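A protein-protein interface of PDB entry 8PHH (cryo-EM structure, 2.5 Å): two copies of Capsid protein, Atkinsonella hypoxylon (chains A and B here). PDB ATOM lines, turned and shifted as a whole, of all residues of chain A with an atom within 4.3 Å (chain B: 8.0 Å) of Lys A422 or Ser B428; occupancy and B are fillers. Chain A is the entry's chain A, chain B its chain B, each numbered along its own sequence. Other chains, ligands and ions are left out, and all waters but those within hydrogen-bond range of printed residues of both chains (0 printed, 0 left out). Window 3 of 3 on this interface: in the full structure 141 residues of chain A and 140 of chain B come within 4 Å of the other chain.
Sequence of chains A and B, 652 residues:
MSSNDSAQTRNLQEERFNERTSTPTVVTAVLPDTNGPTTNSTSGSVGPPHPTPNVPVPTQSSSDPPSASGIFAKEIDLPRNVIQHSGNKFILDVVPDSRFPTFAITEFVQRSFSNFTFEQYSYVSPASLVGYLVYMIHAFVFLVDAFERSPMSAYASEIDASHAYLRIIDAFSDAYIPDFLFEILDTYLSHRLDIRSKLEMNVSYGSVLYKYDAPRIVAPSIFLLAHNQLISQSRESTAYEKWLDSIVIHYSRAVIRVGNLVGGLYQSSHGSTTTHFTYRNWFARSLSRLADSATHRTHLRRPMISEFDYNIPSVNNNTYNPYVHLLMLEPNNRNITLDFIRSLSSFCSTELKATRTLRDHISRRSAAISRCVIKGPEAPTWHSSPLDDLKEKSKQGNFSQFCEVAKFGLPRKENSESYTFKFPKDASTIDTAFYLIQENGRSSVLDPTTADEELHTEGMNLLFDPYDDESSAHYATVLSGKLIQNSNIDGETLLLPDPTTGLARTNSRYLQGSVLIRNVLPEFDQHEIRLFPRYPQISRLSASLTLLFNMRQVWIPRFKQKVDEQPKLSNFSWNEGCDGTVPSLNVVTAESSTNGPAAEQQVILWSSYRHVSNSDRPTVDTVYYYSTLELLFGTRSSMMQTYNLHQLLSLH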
ATOM      1  N   THR A 420      29.979  22.573 -14.571  1.00  0.00           N
ATOM      2  CA  THR A 420      29.881  23.493 -13.446  1.00  0.00           C
ATOM      3  C   THR A 420      28.522  24.170 -13.472  1.00  0.00           C
ATOM      4  O   THR A 420      28.163  24.809 -14.466  1.00  0.00           O
ATOM      5  CB  THR A 420      30.995  24.538 -13.491  1.00  0.00           C
ATOM      6  OG1 THR A 420      32.267  23.882 -13.462  1.00  0.00           O
ATOM      7  CG2 THR A 420      30.891  25.471 -12.299  1.00  0.00           C
ATOM      8  N   PHE A 421      27.772  24.035 -12.384  1.00  0.00           N
ATOM      9  CA  PHE A 421      26.485  24.700 -12.271  1.00  0.00           C
ATOM     10  C   PHE A 421      26.658  26.157 -11.869  1.00  0.00           C
ATOM     11  O   PHE A 421      27.712  26.563 -11.375  1.00  0.00           O
ATOM     12  CB  PHE A 421      25.590  23.984 -11.267  1.00  0.00           C
ATOM     13  CG  PHE A 421      25.005  22.708 -11.782  1.00  0.00           C
ATOM     14  CD1 PHE A 421      23.963  22.736 -12.690  1.00  0.00           C
ATOM     15  CD2 PHE A 421      25.466  21.486 -11.341  1.00  0.00           C
ATOM     16  CE1 PHE A 421      23.409  21.570 -13.165  1.00  0.00           C
ATOM     17  CE2 PHE A 421      24.913  20.315 -11.810  1.00  0.00           C
ATOM     18  CZ  PHE A 421      23.885  20.359 -12.722  1.00  0.00           C
ATOM     19  N   LYS A 422      25.601  26.939 -12.081  1.00  0.00           N
ATOM     20  CA  LYS A 422      25.661  28.397 -11.987  1.00  0.00           C
ATOM     21  C   LYS A 422      24.991  28.845 -10.692  1.00  0.00           C
ATOM     22  O   LYS A 422      23.800  29.162 -10.639  1.00  0.00           O
ATOM     23  CB  LYS A 422      25.004  29.015 -13.212  1.00  0.00           C
ATOM     24  CG  LYS A 422      25.168  30.508 -13.352  1.00  0.00           C
ATOM     25  CD  LYS A 422      24.574  30.962 -14.669  1.00  0.00           C
ATOM     26  CE  LYS A 422      24.756  32.452 -14.874  1.00  0.00           C
ATOM     27  NZ  LYS A 422      24.168  32.907 -16.164  1.00  0.00           N
ATOM     28  N   PHE A 423      25.776  28.867  -9.625  1.00  0.00           N
ATOM     29  CA  PHE A 423      25.274  29.308  -8.336  1.00  0.00           C
ATOM     30  C   PHE A 423      25.456  30.820  -8.203  1.00  0.00           C
ATOM     31  O   PHE A 423      26.501  31.357  -8.573  1.00  0.00           O
ATOM     32  CB  PHE A 423      26.007  28.591  -7.211  1.00  0.00           C
ATOM     33  CG  PHE A 423      25.420  28.822  -5.849  1.00  0.00           C
ATOM     34  CD1 PHE A 423      24.293  28.131  -5.443  1.00  0.00           C
ATOM     35  CD2 PHE A 423      25.993  29.728  -4.974  1.00  0.00           C
ATOM     36  CE1 PHE A 423      23.748  28.335  -4.191  1.00  0.00           C
ATOM     37  CE2 PHE A 423      25.450  29.941  -3.721  1.00  0.00           C
ATOM     38  CZ  PHE A 423      24.325  29.242  -3.331  1.00  0.00           C
ATOM     39  N   PRO A 424      24.449  31.531  -7.689  1.00  0.00           N
ATOM     40  CA  PRO A 424      24.533  32.995  -7.625  1.00  0.00           C
ATOM     41  C   PRO A 424      25.494  33.508  -6.565  1.00  0.00           C
ATOM     42  O   PRO A 424      25.758  32.855  -5.553  1.00  0.00           O
ATOM     43  CB  PRO A 424      23.094  33.404  -7.283  1.00  0.00           C
ATOM     44  CG  PRO A 424      22.537  32.239  -6.573  1.00  0.00           C
ATOM     45  CD  PRO A 424      23.136  31.041  -7.237  1.00  0.00           C
ATOM     46  N   TYR A 435      15.980  25.568  -4.886  1.00  0.00           N
ATOM     47  CA  TYR A 435      17.017  25.620  -5.904  1.00  0.00           C
ATOM     48  C   TYR A 435      17.863  24.362  -5.789  1.00  0.00           C
ATOM     49  O   TYR A 435      18.461  24.105  -4.741  1.00  0.00           O
ATOM     50  CB  TYR A 435      17.847  26.892  -5.737  1.00  0.00           C
ATOM     51  CG  TYR A 435      18.924  27.143  -6.762  1.00  0.00           C
ATOM     52  CD1 TYR A 435      18.617  27.293  -8.102  1.00  0.00           C
ATOM     53  CD2 TYR A 435      20.238  27.341  -6.368  1.00  0.00           C
ATOM     54  CE1 TYR A 435      19.600  27.557  -9.031  1.00  0.00           C
ATOM     55  CE2 TYR A 435      21.221  27.617  -7.287  1.00  0.00           C
ATOM     56  CZ  TYR A 435      20.897  27.722  -8.617  1.00  0.00           C
ATOM     57  OH  TYR A 435      21.875  27.995  -9.541  1.00  0.00           O
ATOM     58  N   PHE B 423      12.737  35.843  -6.335  1.00  0.00           N
ATOM     59  CA  PHE B 423      13.237  35.555  -7.678  1.00  0.00           C
ATOM     60  C   PHE B 423      14.223  36.663  -8.004  1.00  0.00           C
ATOM     61  O   PHE B 423      13.988  37.834  -7.665  1.00  0.00           O
ATOM     62  CB  PHE B 423      12.114  35.492  -8.708  1.00  0.00           C
ATOM     63  CG  PHE B 423      12.548  34.986 -10.047  1.00  0.00           C
ATOM     64  CD1 PHE B 423      12.728  33.632 -10.259  1.00  0.00           C
ATOM     65  CD2 PHE B 423      12.773  35.860 -11.094  1.00  0.00           C
ATOM     66  CE1 PHE B 423      13.124  33.155 -11.490  1.00  0.00           C
ATOM     67  CE2 PHE B 423      13.170  35.390 -12.329  1.00  0.00           C
ATOM     68  CZ  PHE B 423      13.348  34.036 -12.522  1.00  0.00           C
ATOM     69  N   PRO B 424      15.357  36.336  -8.632  1.00  0.00           N
ATOM     70  CA  PRO B 424      16.364  37.365  -8.919  1.00  0.00           C
ATOM     71  C   PRO B 424      15.922  38.372  -9.964  1.00  0.00           C
ATOM     72  O   PRO B 424      15.198  38.029 -10.904  1.00  0.00           O
ATOM     73  CB  PRO B 424      17.561  36.551  -9.424  1.00  0.00           C
ATOM     74  CG  PRO B 424      17.350  35.194  -8.896  1.00  0.00           C
ATOM     75  CD  PRO B 424      15.873  34.984  -8.897  1.00  0.00           C
ATOM     76  N   LYS B 425      16.345  39.627  -9.795  1.00  0.00           N
ATOM     77  CA  LYS B 425      16.135  40.619 -10.839  1.00  0.00           C
ATOM     78  C   LYS B 425      16.983  40.312 -12.063  1.00  0.00           C
ATOM     79  O   LYS B 425      16.577  40.605 -13.192  1.00  0.00           O
ATOM     80  CB  LYS B 425      16.448  42.017 -10.306  1.00  0.00           C
ATOM     81  CG  LYS B 425      15.484  42.501  -9.236  1.00  0.00           C
ATOM     82  CD  LYS B 425      15.838  43.901  -8.760  1.00  0.00           C
ATOM     83  CE  LYS B 425      14.887  44.370  -7.671  1.00  0.00           C
ATOM     84  NZ  LYS B 425      15.228  45.734  -7.183  1.00  0.00           N
ATOM     85  N   ASP B 426      18.155  39.719 -11.858  1.00  0.00           N
ATOM     86  CA  ASP B 426      19.003  39.235 -12.935  1.00  0.00           C
ATOM     87  C   ASP B 426      18.838  37.725 -13.031  1.00  0.00           C
ATOM     88  O   ASP B 426      19.337  36.987 -12.176  1.00  0.00           O
ATOM     89  CB  ASP B 426      20.467  39.601 -12.685  1.00  0.00           C
ATOM     90  CG  ASP B 426      21.348  39.403 -13.912  1.00  0.00           C
ATOM     91  OD1 ASP B 426      20.836  39.002 -14.980  1.00  0.00           O
ATOM     92  OD2 ASP B 426      22.567  39.651 -13.805  1.00  0.00           O
ATOM     93  N   ALA B 427      18.149  37.272 -14.073  1.00  0.00           N
ATOM     94  CA  ALA B 427      17.879  35.856 -14.266  1.00  0.00           C
ATOM     95  C   ALA B 427      19.110  35.065 -14.684  1.00  0.00           C
ATOM     96  O   ALA B 427      19.116  33.839 -14.540  1.00  0.00           O
ATOM     97  CB  ALA B 427      16.771  35.668 -15.306  1.00  0.00           C
ATOM     98  N   SER B 428      20.145  35.727 -15.198  1.00  0.00           N
ATOM     99  CA  SER B 428      21.376  35.049 -15.594  1.00  0.00           C
ATOM    100  C   SER B 428      22.386  35.093 -14.448  1.00  0.00           C
ATOM    101  O   SER B 428      23.536  35.504 -14.593  1.00  0.00           O
ATOM    102  CB  SER B 428      21.941  35.677 -16.864  1.00  0.00           C
ATOM    103  OG  SER B 428      22.367  37.007 -16.626  1.00  0.00           O
ATOM    104  N   THR B 429      21.911  34.673 -13.277  1.00  0.00           N
ATOM    105  CA  THR B 429      22.754  34.454 -12.111  1.00  0.00           C
ATOM    106  C   THR B 429      22.470  33.063 -11.565  1.00  0.00           C
ATOM    107  O   THR B 429      23.243  32.527 -10.768  1.00  0.00           O
ATOM    108  CB  THR B 429      22.506  35.504 -11.023  1.00  0.00           C
ATOM    109  OG1 THR B 429      21.134  35.465 -10.618  1.00  0.00           O
ATOM    110  CG2 THR B 429      22.856  36.904 -11.506  1.00  0.00           C
ATOM    111  N   ILE B 430      21.346  32.478 -11.987  1.00  0.00           N
ATOM    112  CA  ILE B 430      20.933  31.147 -11.565  1.00  0.00           C
ATOM    113  C   ILE B 430      20.599  30.327 -12.802  1.00  0.00           C
ATOM    114  O   ILE B 430      20.359  30.861 -13.886  1.00  0.00           O
ATOM    115  CB  ILE B 430      19.718  31.171 -10.608  1.00  0.00           C
ATOM    116  CG1 ILE B 430      18.502  31.789 -11.296  1.00  0.00           C
ATOM    117  CG2 ILE B 430      20.042  31.909  -9.326  1.00  0.00           C
ATOM    118  CD1 ILE B 430      17.232  31.662 -10.503  1.00  0.00           C
ATOM    119  N   ASP B 431      20.600  29.010 -12.629  1.00  0.00           N
ATOM    120  CA  ASP B 431      20.136  28.095 -13.668  1.00  0.00           C
ATOM    121  C   ASP B 431      18.658  27.776 -13.461  1.00  0.00           C
ATOM    122  O   ASP B 431      18.284  27.014 -12.570  1.00  0.00           O
ATOM    123  CB  ASP B 431      20.987  26.831 -13.673  1.00  0.00           C
ATOM    124  CG  ASP B 431      20.848  26.031 -14.958  1.00  0.00           C
ATOM    125  OD1 ASP B 431      20.075  26.437 -15.851  1.00  0.00           O
ATOM    126  OD2 ASP B 431      21.530  24.993 -15.081  1.00  0.00           O
ATOM    127  N   THR B 432      17.820  28.400 -14.290  1.00  0.00           N
ATOM    128  CA  THR B 432      16.368  28.448 -14.142  1.00  0.00           C
ATOM    129  C   THR B 432      15.725  27.067 -14.189  1.00  0.00           C
ATOM    130  O   THR B 432      14.791  26.784 -13.430  1.00  0.00           O
ATOM    131  CB  THR B 432      15.790  29.359 -15.229  1.00  0.00           C
ATOM    132  OG1 THR B 432      16.354  30.668 -15.095  1.00  0.00           O
ATOM    133  CG2 THR B 432      14.276  29.469 -15.126  1.00  0.00           C
ATOM    134  N   PHE B 434      16.823  24.424 -12.987  1.00  0.00           N
ATOM    135  CA  PHE B 434      17.010  23.793 -11.694  1.00  0.00           C
ATOM    136  C   PHE B 434      16.477  24.645 -10.555  1.00  0.00           C
ATOM    137  O   PHE B 434      16.824  24.400  -9.396  1.00  0.00           O
ATOM    138  CB  PHE B 434      18.494  23.486 -11.484  1.00  0.00           C
ATOM    139  CG  PHE B 434      19.031  22.458 -12.430  1.00  0.00           C
ATOM    140  CD1 PHE B 434      18.892  21.109 -12.158  1.00  0.00           C
ATOM    141  CD2 PHE B 434      19.647  22.841 -13.606  1.00  0.00           C
ATOM    142  CE1 PHE B 434      19.378  20.160 -13.033  1.00  0.00           C
ATOM    143  CE2 PHE B 434      20.132  21.898 -14.485  1.00  0.00           C
ATOM    144  CZ  PHE B 434      19.998  20.556 -14.198  1.00  0.00           C
ATOM    145  N   LYS B 560      25.552  18.976  -6.530  1.00  0.00           N
ATOM    146  CA  LYS B 560      26.764  19.725  -6.239  1.00  0.00           C
ATOM    147  C   LYS B 560      27.013  20.744  -7.342  1.00  0.00           C
ATOM    148  O   LYS B 560      26.431  20.673  -8.426  1.00  0.00           O
ATOM    149  CB  LYS B 560      27.965  18.786  -6.119  1.00  0.00           C
ATOM    150  CG  LYS B 560      27.876  17.767  -5.003  1.00  0.00           C
ATOM    151  CD  LYS B 560      27.902  18.417  -3.637  1.00  0.00           C
ATOM    152  CE  LYS B 560      29.266  18.994  -3.329  1.00  0.00           C
ATOM    153  NZ  LYS B 560      30.298  17.927  -3.218  1.00  0.00           N
ATOM    154  N   GLN B 561      27.894  21.706  -7.064  1.00  0.00           N
ATOM    155  CA  GLN B 561      28.165  22.745  -8.053  1.00  0.00           C
ATOM    156  C   GLN B 561      29.011  22.210  -9.200  1.00  0.00           C
ATOM    157  O   GLN B 561      28.694  22.433 -10.372  1.00  0.00           O
ATOM    158  CB  GLN B 561      28.840  23.945  -7.398  1.00  0.00           C
ATOM    159  CG  GLN B 561      27.937  24.725  -6.475  1.00  0.00           C
ATOM    160  CD  GLN B 561      28.615  25.938  -5.887  1.00  0.00           C
ATOM    161  OE1 GLN B 561      29.790  26.192  -6.146  1.00  0.00           O
ATOM    162  NE2 GLN B 561      27.881  26.692  -5.081  1.00  0.00           N
ATOM    163  N   LYS B 562      30.089  21.501  -8.886  1.00  0.00           N
ATOM    164  CA  LYS B 562      30.963  20.909  -9.892  1.00  0.00           C
ATOM    165  C   LYS B 562      30.644  19.422  -9.983  1.00  0.00           C
ATOM    166  O   LYS B 562      30.886  18.670  -9.035  1.00  0.00           O
ATOM    167  CB  LYS B 562      32.429  21.141  -9.541  1.00  0.00           C
ATOM    168  CG  LYS B 562      32.844  22.599  -9.583  1.00  0.00           C
ATOM    169  CD  LYS B 562      34.294  22.778  -9.182  1.00  0.00           C
ATOM    170  CE  LYS B 562      35.228  22.264 -10.264  1.00  0.00           C
ATOM    171  NZ  LYS B 562      35.166  23.098 -11.496  1.00  0.00           N
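Positions printed for both chains: 423 and 424. Of the 16 pairs that touch across the chains among the printed residues, none has its exchanged pair printed and touching as well.
The side-chain carboxylate (OD1) of Asp B426 lies within hydrogen-bond range of the side-chain hydroxyl (OG) of Ser B428 (3.0 Å). O of Asp B426 sits at hydrogen-bond distance from OG1 of Thr B429 (2.8 Å). O of Lys A422 lies within hydrogen-bond range of OH of Tyr A435, 2.5 Å away.
NZ of Lys A422 sits at hydrogen-bond distance from O of Ser B428, at 3.1 Å. OH of Tyr A435 sits at hydrogen-bond distance from N of Asp B431, 3.5 Å away. N of Phe A421 sits at hydrogen-bond distance from O of Gln B561, 2.7 Å away. O of Lys A422 lies close to O of Thr B429 (3.4 Å). The backbone carbonyl oxygen of Thr B429 lies close to the backbone nitrogen of Pro A424 (3.5 Å).
Ser B428 touches one residue of chain A. Printed residues of chain B within 4 Å of Thr A420: Gln B561 (3.5 Å) and Lys B562 (3.6 Å). Of the printed residues of chain A, Phe B434 touches Phe A421 and Tyr A435. Of the printed residues of chain A, Lys B562 touches Thr A420 (3.6 Å). Of the printed residues of chain B, Phe A423 touches Thr B429 and Gln B561. The nearest residue of chain B that does not touch Lys A422 is Ala B427 (5.4 Å). The nearest printed residue of chain A that does not touch Ser B428 is Pro A424 (7.4 Å). The nearest printed residue of chain B that does not touch Tyr A435 is Thr B429 (4.9 Å).
Of the 14 printed residues of chain B, 8 touch a printed residue of chain A. Hydrophobic or aromatic side chains of chain B that line the printed part of chain A: Ile B430 and Phe B434. Along chain B the printed residues that touch a printed residue of chain A span positions 428 to 562. Of the 6 printed residues of chain A, 6 touch a printed residue of chain B. Printed residues of chain A that touch a printed residue of chain B: Thr A420, Phe A421, Lys A422, Phe A423, Pro A424 and Tyr A435. Hydrophobic or aromatic side chains of chain A within 4 Å of the printed part of chain B: Phe A421, Phe A423, Pro A424 and Tyr A435.
Thr A420 touches Gln B561 (CA to O, 3.5 Å). Thr A420 touches Lys B562 (OG1 to NZ, 3.6 Å). Phe A421 touches Lys B560. O of Lys A422 touches CA of Ile B430, 3.6 Å away. N of Asp B431 touches O of Lys A422 (3.8 Å). O of Thr B429 touches C of Phe A423, 3.8 Å away. Gln B561 touches Phe A423 (NE2 to CG, 3.3 Å). CG of Pro A424 touches CG2 of Ile B430, 3.7 Å away. Ile B430 touches Tyr A435. Tyr A435 touches Phe B434 (CD1 to O, 3.6 Å).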
